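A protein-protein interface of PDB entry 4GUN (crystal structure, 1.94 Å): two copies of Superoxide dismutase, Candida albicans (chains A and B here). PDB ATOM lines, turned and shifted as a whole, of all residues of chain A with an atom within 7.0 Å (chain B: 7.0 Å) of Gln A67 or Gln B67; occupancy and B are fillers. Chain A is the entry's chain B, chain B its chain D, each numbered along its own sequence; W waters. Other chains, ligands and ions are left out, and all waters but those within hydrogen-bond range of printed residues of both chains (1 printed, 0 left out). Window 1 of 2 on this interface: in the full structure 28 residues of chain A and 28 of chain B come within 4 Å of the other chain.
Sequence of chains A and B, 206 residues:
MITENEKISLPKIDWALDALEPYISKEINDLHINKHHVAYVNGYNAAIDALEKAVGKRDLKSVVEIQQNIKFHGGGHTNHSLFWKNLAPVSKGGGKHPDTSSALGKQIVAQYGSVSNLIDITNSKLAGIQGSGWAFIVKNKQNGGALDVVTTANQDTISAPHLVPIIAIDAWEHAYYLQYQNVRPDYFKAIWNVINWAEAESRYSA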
ATOM      1  N   ALA A  47     -23.437   2.718  -1.932  1.00  0.00           N
ATOM      2  CA  ALA A  47     -22.582   3.384  -0.939  1.00  0.00           C
ATOM      3  C   ALA A  47     -23.368   3.850   0.313  1.00  0.00           C
ATOM      4  O   ALA A  47     -22.901   3.654   1.443  1.00  0.00           O
ATOM      5  CB  ALA A  47     -21.826   4.539  -1.573  1.00  0.00           C
ATOM      6  N   ILE A  48     -24.570   4.413   0.117  1.00  0.00           N
ATOM      7  CA  ILE A  48     -25.441   4.839   1.222  1.00  0.00           C
ATOM      8  C   ILE A  48     -25.793   3.630   2.091  1.00  0.00           C
ATOM      9  O   ILE A  48     -25.737   3.724   3.313  1.00  0.00           O
ATOM     10  CB  ILE A  48     -26.685   5.633   0.697  1.00  0.00           C
ATOM     11  CG1 ILE A  48     -26.266   7.004   0.150  1.00  0.00           C
ATOM     12  CG2 ILE A  48     -27.808   5.791   1.748  1.00  0.00           C
ATOM     13  CD1 ILE A  48     -25.441   7.955   1.089  1.00  0.00           C
ATOM     14  N   LEU A  51     -22.647   2.554   3.937  1.00  0.00           N
ATOM     15  CA  LEU A  51     -22.353   3.611   4.915  1.00  0.00           C
ATOM     16  C   LEU A  51     -23.146   3.452   6.200  1.00  0.00           C
ATOM     17  O   LEU A  51     -22.565   3.491   7.282  1.00  0.00           O
ATOM     18  CB  LEU A  51     -22.625   4.992   4.310  1.00  0.00           C
ATOM     19  CG  LEU A  51     -22.041   6.232   5.008  1.00  0.00           C
ATOM     20  CD1 LEU A  51     -23.038   6.878   5.924  1.00  0.00           C
ATOM     21  CD2 LEU A  51     -20.695   5.959   5.668  1.00  0.00           C
ATOM     22  N   VAL A  55     -21.609   2.892   9.813  1.00  0.00           N
ATOM     23  CA  VAL A  55     -21.896   3.943  10.820  1.00  0.00           C
ATOM     24  C   VAL A  55     -22.611   3.326  12.043  1.00  0.00           C
ATOM     25  O   VAL A  55     -22.291   3.669  13.182  1.00  0.00           O
ATOM     26  CB  VAL A  55     -22.675   5.154  10.213  1.00  0.00           C
ATOM     27  CG1 VAL A  55     -23.356   6.010  11.286  1.00  0.00           C
ATOM     28  CG2 VAL A  55     -21.763   6.017   9.353  1.00  0.00           C
ATOM     29  N   LEU A  60     -15.294   2.835  11.860  1.00  0.00           N
ATOM     30  CA  LEU A  60     -14.740   4.033  11.242  1.00  0.00           C
ATOM     31  C   LEU A  60     -13.786   3.799  10.091  1.00  0.00           C
ATOM     32  O   LEU A  60     -13.792   4.590   9.140  1.00  0.00           O
ATOM     33  CB  LEU A  60     -14.224   5.048  12.280  1.00  0.00           C
ATOM     34  CG  LEU A  60     -15.278   6.044  12.801  1.00  0.00           C
ATOM     35  CD1 LEU A  60     -16.381   5.356  13.643  1.00  0.00           C
ATOM     36  CD2 LEU A  60     -14.634   7.165  13.584  1.00  0.00           C
ATOM     37  N   SER A  62     -14.063   1.454   7.738  1.00  0.00           N
ATOM     38  CA  SER A  62     -14.963   1.261   6.600  1.00  0.00           C
ATOM     39  C   SER A  62     -15.648   2.575   6.250  1.00  0.00           C
ATOM     40  O   SER A  62     -15.648   2.955   5.079  1.00  0.00           O
ATOM     41  CB  SER A  62     -16.007   0.196   6.918  1.00  0.00           C
ATOM     42  OG  SER A  62     -15.374  -1.029   7.252  1.00  0.00           O
ATOM     43  N   VAL A  63     -16.199   3.279   7.269  1.00  0.00           N
ATOM     44  CA  VAL A  63     -16.866   4.578   7.122  1.00  0.00           C
ATOM     45  C   VAL A  63     -15.991   5.529   6.289  1.00  0.00           C
ATOM     46  O   VAL A  63     -16.437   6.011   5.242  1.00  0.00           O
ATOM     47  CB  VAL A  63     -17.249   5.166   8.503  1.00  0.00           C
ATOM     48  CG1 VAL A  63     -17.480   6.674   8.443  1.00  0.00           C
ATOM     49  CG2 VAL A  63     -18.481   4.469   9.061  1.00  0.00           C
ATOM     50  N   VAL A  64     -14.722   5.711   6.712  1.00  0.00           N
ATOM     51  CA  VAL A  64     -13.753   6.586   6.045  1.00  0.00           C
ATOM     52  C   VAL A  64     -13.485   6.156   4.591  1.00  0.00           C
ATOM     53  O   VAL A  64     -13.351   7.018   3.716  1.00  0.00           O
ATOM     54  CB  VAL A  64     -12.488   6.747   6.921  1.00  0.00           C
ATOM     55  CG1 VAL A  64     -11.221   6.920   6.094  1.00  0.00           C
ATOM     56  CG2 VAL A  64     -12.666   7.883   7.919  1.00  0.00           C
ATOM     57  N   GLU A  65     -13.440   4.821   4.339  1.00  0.00           N
ATOM     58  CA  GLU A  65     -13.259   4.244   3.013  1.00  0.00           C
ATOM     59  C   GLU A  65     -14.496   4.502   2.125  1.00  0.00           C
ATOM     60  O   GLU A  65     -14.319   4.905   0.975  1.00  0.00           O
ATOM     61  CB  GLU A  65     -12.922   2.737   3.125  1.00  0.00           C
ATOM     62  CG  GLU A  65     -12.594   2.027   1.820  1.00  0.00           C
ATOM     63  CD  GLU A  65     -11.224   2.233   1.188  1.00  0.00           C
ATOM     64  OE1 GLU A  65     -10.457   3.111   1.648  1.00  0.00           O
ATOM     65  OE2 GLU A  65     -10.924   1.509   0.211  1.00  0.00           O
ATOM     66  N   ILE A  66     -15.738   4.312   2.668  1.00  0.00           N
ATOM     67  CA  ILE A  66     -17.008   4.479   1.936  1.00  0.00           C
ATOM     68  C   ILE A  66     -17.248   5.933   1.472  1.00  0.00           C
ATOM     69  O   ILE A  66     -17.732   6.136   0.359  1.00  0.00           O
ATOM     70  CB  ILE A  66     -18.224   3.824   2.688  1.00  0.00           C
ATOM     71  CG1 ILE A  66     -17.952   2.324   3.032  1.00  0.00           C
ATOM     72  CG2 ILE A  66     -19.557   3.957   1.897  1.00  0.00           C
ATOM     73  CD1 ILE A  66     -18.807   1.762   4.271  1.00  0.00           C
ATOM     74  N   GLN A  67     -16.824   6.937   2.279  1.00  0.00           N
ATOM     75  CA  GLN A  67     -16.964   8.369   1.980  1.00  0.00           C
ATOM     76  C   GLN A  67     -16.581   8.722   0.545  1.00  0.00           C
ATOM     77  O   GLN A  67     -17.288   9.505  -0.073  1.00  0.00           O
ATOM     78  CB  GLN A  67     -16.119   9.251   2.935  1.00  0.00           C
ATOM     79  CG  GLN A  67     -16.398   9.105   4.418  1.00  0.00           C
ATOM     80  CD  GLN A  67     -17.864   9.044   4.738  1.00  0.00           C
ATOM     81  OE1 GLN A  67     -18.610  10.002   4.551  1.00  0.00           O
ATOM     82  NE2 GLN A  67     -18.293   7.930   5.277  1.00  0.00           N
ATOM     83  N   GLN A  68     -15.473   8.151   0.021  1.00  0.00           N
ATOM     84  CA  GLN A  68     -15.026   8.407  -1.347  1.00  0.00           C
ATOM     85  C   GLN A  68     -16.065   7.982  -2.396  1.00  0.00           C
ATOM     86  O   GLN A  68     -16.304   8.720  -3.344  1.00  0.00           O
ATOM     87  CB  GLN A  68     -13.641   7.780  -1.616  1.00  0.00           C
ATOM     88  CG  GLN A  68     -13.039   8.131  -2.986  1.00  0.00           C
ATOM     89  CD  GLN A  68     -12.856   9.609  -3.267  1.00  0.00           C
ATOM     90  OE1 GLN A  68     -12.532  10.410  -2.390  1.00  0.00           O
ATOM     91  NE2 GLN A  68     -13.060  10.013  -4.519  1.00  0.00           N
ATOM     92  N   ASN A  69     -16.689   6.810  -2.213  1.00  0.00           N
ATOM     93  CA  ASN A  69     -17.728   6.317  -3.119  1.00  0.00           C
ATOM     94  C   ASN A  69     -18.993   7.156  -3.052  1.00  0.00           C
ATOM     95  O   ASN A  69     -19.625   7.360  -4.085  1.00  0.00           O
ATOM     96  CB  ASN A  69     -17.983   4.819  -2.942  1.00  0.00           C
ATOM     97  CG  ASN A  69     -16.822   3.962  -3.407  1.00  0.00           C
ATOM     98  OD1 ASN A  69     -15.806   4.461  -3.897  1.00  0.00           O
ATOM     99  ND2 ASN A  69     -16.946   2.648  -3.270  1.00  0.00           N
ATOM    100  N   ILE A  70     -19.306   7.737  -1.875  1.00  0.00           N
ATOM    101  CA  ILE A  70     -20.463   8.632  -1.740  1.00  0.00           C
ATOM    102  C   ILE A  70     -20.213   9.891  -2.552  1.00  0.00           C
ATOM    103  O   ILE A  70     -21.095  10.344  -3.284  1.00  0.00           O
ATOM    104  CB  ILE A  70     -20.820   8.958  -0.264  1.00  0.00           C
ATOM    105  CG1 ILE A  70     -21.401   7.716   0.435  1.00  0.00           C
ATOM    106  CG2 ILE A  70     -21.862  10.108  -0.199  1.00  0.00           C
ATOM    107  CD1 ILE A  70     -20.827   7.448   1.727  1.00  0.00           C
ATOM    108  N   LYS A  71     -19.006  10.462  -2.392  1.00  0.00           N
ATOM    109  CA  LYS A  71     -18.562  11.684  -3.051  1.00  0.00           C
ATOM    110  C   LYS A  71     -18.545  11.461  -4.557  1.00  0.00           C
ATOM    111  O   LYS A  71     -19.154  12.243  -5.290  1.00  0.00           O
ATOM    112  CB  LYS A  71     -17.160  12.074  -2.492  1.00  0.00           C
ATOM    113  CG  LYS A  71     -16.513  13.323  -3.093  1.00  0.00           C
ATOM    114  CD  LYS A  71     -15.169  13.546  -2.414  1.00  0.00           C
ATOM    115  CE  LYS A  71     -14.154  14.260  -3.269  1.00  0.00           C
ATOM    116  NZ  LYS A  71     -14.179  15.731  -3.051  1.00  0.00           N
ATOM    117  N   PHE A  72     -17.874  10.383  -5.022  1.00  0.00           N
ATOM    118  CA  PHE A  72     -17.782  10.086  -6.459  1.00  0.00           C
ATOM    119  C   PHE A  72     -19.144   9.856  -7.108  1.00  0.00           C
ATOM    120  O   PHE A  72     -19.485  10.543  -8.065  1.00  0.00           O
ATOM    121  CB  PHE A  72     -16.820   8.902  -6.726  1.00  0.00           C
ATOM    122  CG  PHE A  72     -16.619   8.548  -8.181  1.00  0.00           C
ATOM    123  CD1 PHE A  72     -15.837   9.348  -9.009  1.00  0.00           C
ATOM    124  CD2 PHE A  72     -17.154   7.377  -8.708  1.00  0.00           C
ATOM    125  CE1 PHE A  72     -15.615   8.996 -10.346  1.00  0.00           C
ATOM    126  CE2 PHE A  72     -16.923   7.022 -10.043  1.00  0.00           C
ATOM    127  CZ  PHE A  72     -16.150   7.831 -10.849  1.00  0.00           C
ATOM    128  N   TYR B  44     -16.866  14.412  14.335  1.00  0.00           N
ATOM    129  CA  TYR B  44     -17.438  13.215  13.722  1.00  0.00           C
ATOM    130  C   TYR B  44     -18.901  13.061  14.112  1.00  0.00           C
ATOM    131  O   TYR B  44     -19.733  12.845  13.237  1.00  0.00           O
ATOM    132  CB  TYR B  44     -16.639  11.933  14.063  1.00  0.00           C
ATOM    133  CG  TYR B  44     -17.226  10.661  13.482  1.00  0.00           C
ATOM    134  CD1 TYR B  44     -16.951  10.276  12.171  1.00  0.00           C
ATOM    135  CD2 TYR B  44     -18.062   9.847  14.239  1.00  0.00           C
ATOM    136  CE1 TYR B  44     -17.500   9.110  11.625  1.00  0.00           C
ATOM    137  CE2 TYR B  44     -18.625   8.686  13.703  1.00  0.00           C
ATOM    138  CZ  TYR B  44     -18.340   8.319  12.396  1.00  0.00           C
ATOM    139  OH  TYR B  44     -18.868   7.152  11.889  1.00  0.00           O
ATOM    140  N   ALA B  47     -20.978  15.565  12.188  1.00  0.00           N
ATOM    141  CA  ALA B  47     -20.982  15.231  10.752  1.00  0.00           C
ATOM    142  C   ALA B  47     -21.939  14.079  10.441  1.00  0.00           C
ATOM    143  O   ALA B  47     -22.631  14.127   9.421  1.00  0.00           O
ATOM    144  CB  ALA B  47     -19.574  14.898  10.270  1.00  0.00           C
ATOM    145  N   ILE B  48     -22.015  13.076  11.333  1.00  0.00           N
ATOM    146  CA  ILE B  48     -22.934  11.939  11.173  1.00  0.00           C
ATOM    147  C   ILE B  48     -24.391  12.383  11.319  1.00  0.00           C
ATOM    148  O   ILE B  48     -25.252  11.914  10.569  1.00  0.00           O
ATOM    149  CB  ILE B  48     -22.553  10.746  12.107  1.00  0.00           C
ATOM    150  CG1 ILE B  48     -21.305  10.006  11.588  1.00  0.00           C
ATOM    151  CG2 ILE B  48     -23.744   9.765  12.378  1.00  0.00           C
ATOM    152  CD1 ILE B  48     -21.297   9.590  10.071  1.00  0.00           C
ATOM    153  N   LEU B  51     -25.250  14.312   8.177  1.00  0.00           N
ATOM    154  CA  LEU B  51     -25.324  13.369   7.062  1.00  0.00           C
ATOM    155  C   LEU B  51     -26.666  12.618   6.997  1.00  0.00           C
ATOM    156  O   LEU B  51     -27.251  12.538   5.914  1.00  0.00           O
ATOM    157  CB  LEU B  51     -24.124  12.392   7.117  1.00  0.00           C
ATOM    158  CG  LEU B  51     -23.747  11.555   5.874  1.00  0.00           C
ATOM    159  CD1 LEU B  51     -24.317  10.169   5.934  1.00  0.00           C
ATOM    160  CD2 LEU B  51     -23.974  12.291   4.550  1.00  0.00           C
ATOM    161  N   VAL B  55     -29.093  12.829   3.824  1.00  0.00           N
ATOM    162  CA  VAL B  55     -29.311  11.558   3.106  1.00  0.00           C
ATOM    163  C   VAL B  55     -30.819  11.283   3.007  1.00  0.00           C
ATOM    164  O   VAL B  55     -31.323  10.959   1.922  1.00  0.00           O
ATOM    165  CB  VAL B  55     -28.522  10.354   3.744  1.00  0.00           C
ATOM    166  CG1 VAL B  55     -29.122   8.992   3.375  1.00  0.00           C
ATOM    167  CG2 VAL B  55     -27.044  10.398   3.363  1.00  0.00           C
ATOM    168  N   SER B  62     -25.656  18.607  -0.106  1.00  0.00           N
ATOM    169  CA  SER B  62     -25.213  18.592   1.303  1.00  0.00           C
ATOM    170  C   SER B  62     -24.461  17.284   1.625  1.00  0.00           C
ATOM    171  O   SER B  62     -23.413  17.319   2.283  1.00  0.00           O
ATOM    172  CB  SER B  62     -26.393  18.765   2.260  1.00  0.00           C
ATOM    173  OG  SER B  62     -26.607  20.126   2.591  1.00  0.00           O
ATOM    174  N   VAL B  63     -25.011  16.144   1.160  1.00  0.00           N
ATOM    175  CA  VAL B  63     -24.424  14.808   1.332  1.00  0.00           C
ATOM    176  C   VAL B  63     -22.934  14.847   0.892  1.00  0.00           C
ATOM    177  O   VAL B  63     -22.042  14.479   1.672  1.00  0.00           O
ATOM    178  CB  VAL B  63     -25.243  13.735   0.572  1.00  0.00           C
ATOM    179  CG1 VAL B  63     -24.495  12.407   0.476  1.00  0.00           C
ATOM    180  CG2 VAL B  63     -26.607  13.532   1.210  1.00  0.00           C
ATOM    181  N   VAL B  64     -22.688  15.350  -0.322  1.00  0.00           N
ATOM    182  CA  VAL B  64     -21.346  15.485  -0.910  1.00  0.00           C
ATOM    183  C   VAL B  64     -20.407  16.357  -0.082  1.00  0.00           C
ATOM    184  O   VAL B  64     -19.277  15.948   0.171  1.00  0.00           O
ATOM    185  CB  VAL B  64     -21.407  15.870  -2.413  1.00  0.00           C
ATOM    186  CG1 VAL B  64     -20.088  16.461  -2.901  1.00  0.00           C
ATOM    187  CG2 VAL B  64     -21.797  14.661  -3.258  1.00  0.00           C
ATOM    188  N   GLU B  65     -20.900  17.519   0.387  1.00  0.00           N
ATOM    189  CA  GLU B  65     -20.151  18.461   1.209  1.00  0.00           C
ATOM    190  C   GLU B  65     -19.725  17.847   2.558  1.00  0.00           C
ATOM    191  O   GLU B  65     -18.561  17.987   2.946  1.00  0.00           O
ATOM    192  CB  GLU B  65     -20.975  19.758   1.397  1.00  0.00           C
ATOM    193  CG  GLU B  65     -20.244  20.897   2.099  1.00  0.00           C
ATOM    194  CD  GLU B  65     -19.234  21.718   1.305  1.00  0.00           C
ATOM    195  OE1 GLU B  65     -18.810  21.279   0.211  1.00  0.00           O
ATOM    196  OE2 GLU B  65     -18.842  22.799   1.802  1.00  0.00           O
ATOM    197  N   ILE B  66     -20.664  17.143   3.242  1.00  0.00           N
ATOM    198  CA  ILE B  66     -20.509  16.515   4.565  1.00  0.00           C
ATOM    199  C   ILE B  66     -19.472  15.382   4.545  1.00  0.00           C
ATOM    200  O   ILE B  66     -18.804  15.169   5.550  1.00  0.00           O
ATOM    201  CB  ILE B  66     -21.895  16.040   5.139  1.00  0.00           C
ATOM    202  CG1 ILE B  66     -22.849  17.232   5.382  1.00  0.00           C
ATOM    203  CG2 ILE B  66     -21.724  15.276   6.440  1.00  0.00           C
ATOM    204  CD1 ILE B  66     -24.377  16.849   5.486  1.00  0.00           C
ATOM    205  N   GLN B  67     -19.334  14.662   3.415  1.00  0.00           N
ATOM    206  CA  GLN B  67     -18.365  13.558   3.252  1.00  0.00           C
ATOM    207  C   GLN B  67     -16.960  13.907   3.711  1.00  0.00           C
ATOM    208  O   GLN B  67     -16.314  13.081   4.358  1.00  0.00           O
ATOM    209  CB  GLN B  67     -18.302  13.078   1.784  1.00  0.00           C
ATOM    210  CG  GLN B  67     -19.582  12.486   1.268  1.00  0.00           C
ATOM    211  CD  GLN B  67     -20.220  11.568   2.277  1.00  0.00           C
ATOM    212  OE1 GLN B  67     -21.224  11.893   2.924  1.00  0.00           O
ATOM    213  NE2 GLN B  67     -19.635  10.409   2.440  1.00  0.00           N
ATOM    214  N   GLN B  68     -16.481  15.121   3.365  1.00  0.00           N
ATOM    215  CA  GLN B  68     -15.145  15.603   3.734  1.00  0.00           C
ATOM    216  C   GLN B  68     -15.003  15.708   5.255  1.00  0.00           C
ATOM    217  O   GLN B  68     -13.960  15.348   5.781  1.00  0.00           O
ATOM    218  CB  GLN B  68     -14.826  16.945   3.039  1.00  0.00           C
ATOM    219  CG  GLN B  68     -13.340  17.405   3.099  1.00  0.00           C
ATOM    220  CD  GLN B  68     -12.293  16.340   2.808  1.00  0.00           C
ATOM    221  OE1 GLN B  68     -11.308  16.176   3.549  1.00  0.00           O
ATOM    222  NE2 GLN B  68     -12.452  15.615   1.714  1.00  0.00           N
ATOM    223  N   ASN B  69     -16.069  16.145   5.966  1.00  0.00           N
ATOM    224  CA  ASN B  69     -15.996  16.257   7.422  1.00  0.00           C
ATOM    225  C   ASN B  69     -16.003  14.896   8.074  1.00  0.00           C
ATOM    226  O   ASN B  69     -15.357  14.702   9.102  1.00  0.00           O
ATOM    227  CB  ASN B  69     -17.071  17.193   7.968  1.00  0.00           C
ATOM    228  CG  ASN B  69     -16.687  18.650   7.855  1.00  0.00           C
ATOM    229  OD1 ASN B  69     -16.010  19.062   6.912  1.00  0.00           O
ATOM    230  ND2 ASN B  69     -17.060  19.452   8.851  1.00  0.00           N
ATOM    231  N   ILE B  70     -16.677  13.929   7.441  1.00  0.00           N
ATOM    232  CA  ILE B  70     -16.690  12.565   7.936  1.00  0.00           C
ATOM    233  C   ILE B  70     -15.298  11.970   7.818  1.00  0.00           C
ATOM    234  O   ILE B  70     -14.766  11.490   8.808  1.00  0.00           O
ATOM    235  CB  ILE B  70     -17.782  11.699   7.276  1.00  0.00           C
ATOM    236  CG1 ILE B  70     -19.170  12.298   7.579  1.00  0.00           C
ATOM    237  CG2 ILE B  70     -17.680  10.257   7.805  1.00  0.00           C
ATOM    238  CD1 ILE B  70     -20.262  11.853   6.642  1.00  0.00           C
ATOM    239  N   LYS B  71     -14.696  12.057   6.634  1.00  0.00           N
ATOM    240  CA  LYS B  71     -13.333  11.586   6.361  1.00  0.00           C
ATOM    241  C   LYS B  71     -12.327  12.204   7.342  1.00  0.00           C
ATOM    242  O   LYS B  71     -11.513  11.482   7.913  1.00  0.00           O
ATOM    243  CB  LYS B  71     -12.933  11.899   4.897  1.00  0.00           C
ATOM    244  CG  LYS B  71     -11.507  11.453   4.533  1.00  0.00           C
ATOM    245  CD  LYS B  71     -11.226  11.414   3.027  1.00  0.00           C
ATOM    246  CE  LYS B  71     -11.002  12.760   2.371  1.00  0.00           C
ATOM    247  NZ  LYS B  71      -9.672  13.353   2.687  1.00  0.00           N
ATOM    248  N   PHE B  72     -12.409  13.528   7.544  1.00  0.00           N
ATOM    249  CA  PHE B  72     -11.484  14.274   8.396  1.00  0.00           C
ATOM    250  C   PHE B  72     -11.604  13.984   9.884  1.00  0.00           C
ATOM    251  O   PHE B  72     -10.595  13.704  10.533  1.00  0.00           O
ATOM    252  CB  PHE B  72     -11.585  15.787   8.112  1.00  0.00           C
ATOM    253  CG  PHE B  72     -10.602  16.656   8.857  1.00  0.00           C
ATOM    254  CD1 PHE B  72      -9.274  16.743   8.449  1.00  0.00           C
ATOM    255  CD2 PHE B  72     -11.004  17.397   9.966  1.00  0.00           C
ATOM    256  CE1 PHE B  72      -8.365  17.553   9.135  1.00  0.00           C
ATOM    257  CE2 PHE B  72     -10.096  18.223  10.646  1.00  0.00           C
ATOM    258  CZ  PHE B  72      -8.788  18.312  10.212  1.00  0.00           C
HETATM  259  O   HOH W   1     -20.464   5.668  13.780  1.00  0.00           O
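Val B55 touches Ile A48. Leu A51 touches Leu B51 (CD1 to CD1, 3.5 Å). Ile B48 touches Val A55. OH of Tyr B44 touches CD1 of Leu A60, at 3.5 Å. Tyr B44 touches Val A63. Val A63 touches Ile B70 (CG1 to CG2, 3.6 Å). CG2 of Val A64 touches O of Lys B71, 3.8 Å away. Ile B70 touches Gln A67. Ile A70 touches Val B63 (CG2 to CG1, 3.6 Å). Ile A70 touches Gln B67 (CD1 to NE2, 3.3 Å).
Printed residues of chain A that touch a printed residue of chain B: Ile A48, Leu A51, Val A55, Leu A60, Val A63, Val A64, Gln A67 and Ile A70. Hydrophobic or aromatic side chains of chain A that line the printed part of chain B: Ile A48, Leu A51, Val A55, Leu A60, Val A63, Val A64 and Ile A70. Along chain A the printed residues that touch a printed residue of chain B span positions 48 to 70. Hydrophobic or aromatic side chains of chain B that line the printed part of chain A: Tyr B44, Ile B48, Leu B51, Val B55, Val B63 and Ile B70.
NE2 of Gln A67 sits at hydrogen-bond distance from O of Val A63. O of Val B63 lies close to OE1 of Gln B67, 3.0 Å away. The side-chain amide oxygen of Gln B68 sits at hydrogen-bond distance from the side-chain amino group of Lys B71, 3.4 Å away.
The side-chain amide oxygen of Gln A67 sits close to the side-chain amide nitrogen of Gln B67 (2.4 Å).
Water W1 lies within hydrogen-bond range of O of Val A55 (2.8 Å) and OH of Tyr B44 (2.9 Å).
Ile A48 touches Val B55, and with the chains exchanged Val A55 touches Ile B48. Val A63 touches Ile B70, and with the chains exchanged Ile A70 touches Val B63. Val A64 touches Lys B71, but with the chains exchanged Lys A71 does not touch Val B64 (4.1 Å). Gln A67 touches its own counterpart, Gln B67. Of the 11 pairs that touch across the chains among the printed residues, 8 have their exchanged pair printed and touching as well.
Of chain B, only Gln B67 and Ile B70 come within 4 Å of Gln A67. Gln B67 touches just these residues of chain A: Gln A67 and Ile A70. Printed residues of chain B within 4 Å of Ile A70: Val B63 and Gln B67. Printed residues of chain A within 4 Å of Ile B48: Val A55 (3.7 Å). Printed residues of chain A within 4 Å of Ile B70: Val A63 and Gln A67. Gln B68 touches none of the printed residues of chain A. Glu A65 touches none of the printed residues of chain B. The nearest residue of chain B that does not touch Gln A67 is Lys B71 (4.1 Å). The nearest residue of chain A that does not touch Gln B67 is Lys A71 (4.2 Å). The nearest printed residue of chain A that does not touch Lys B71 is Gln A67 (4.1 Å).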
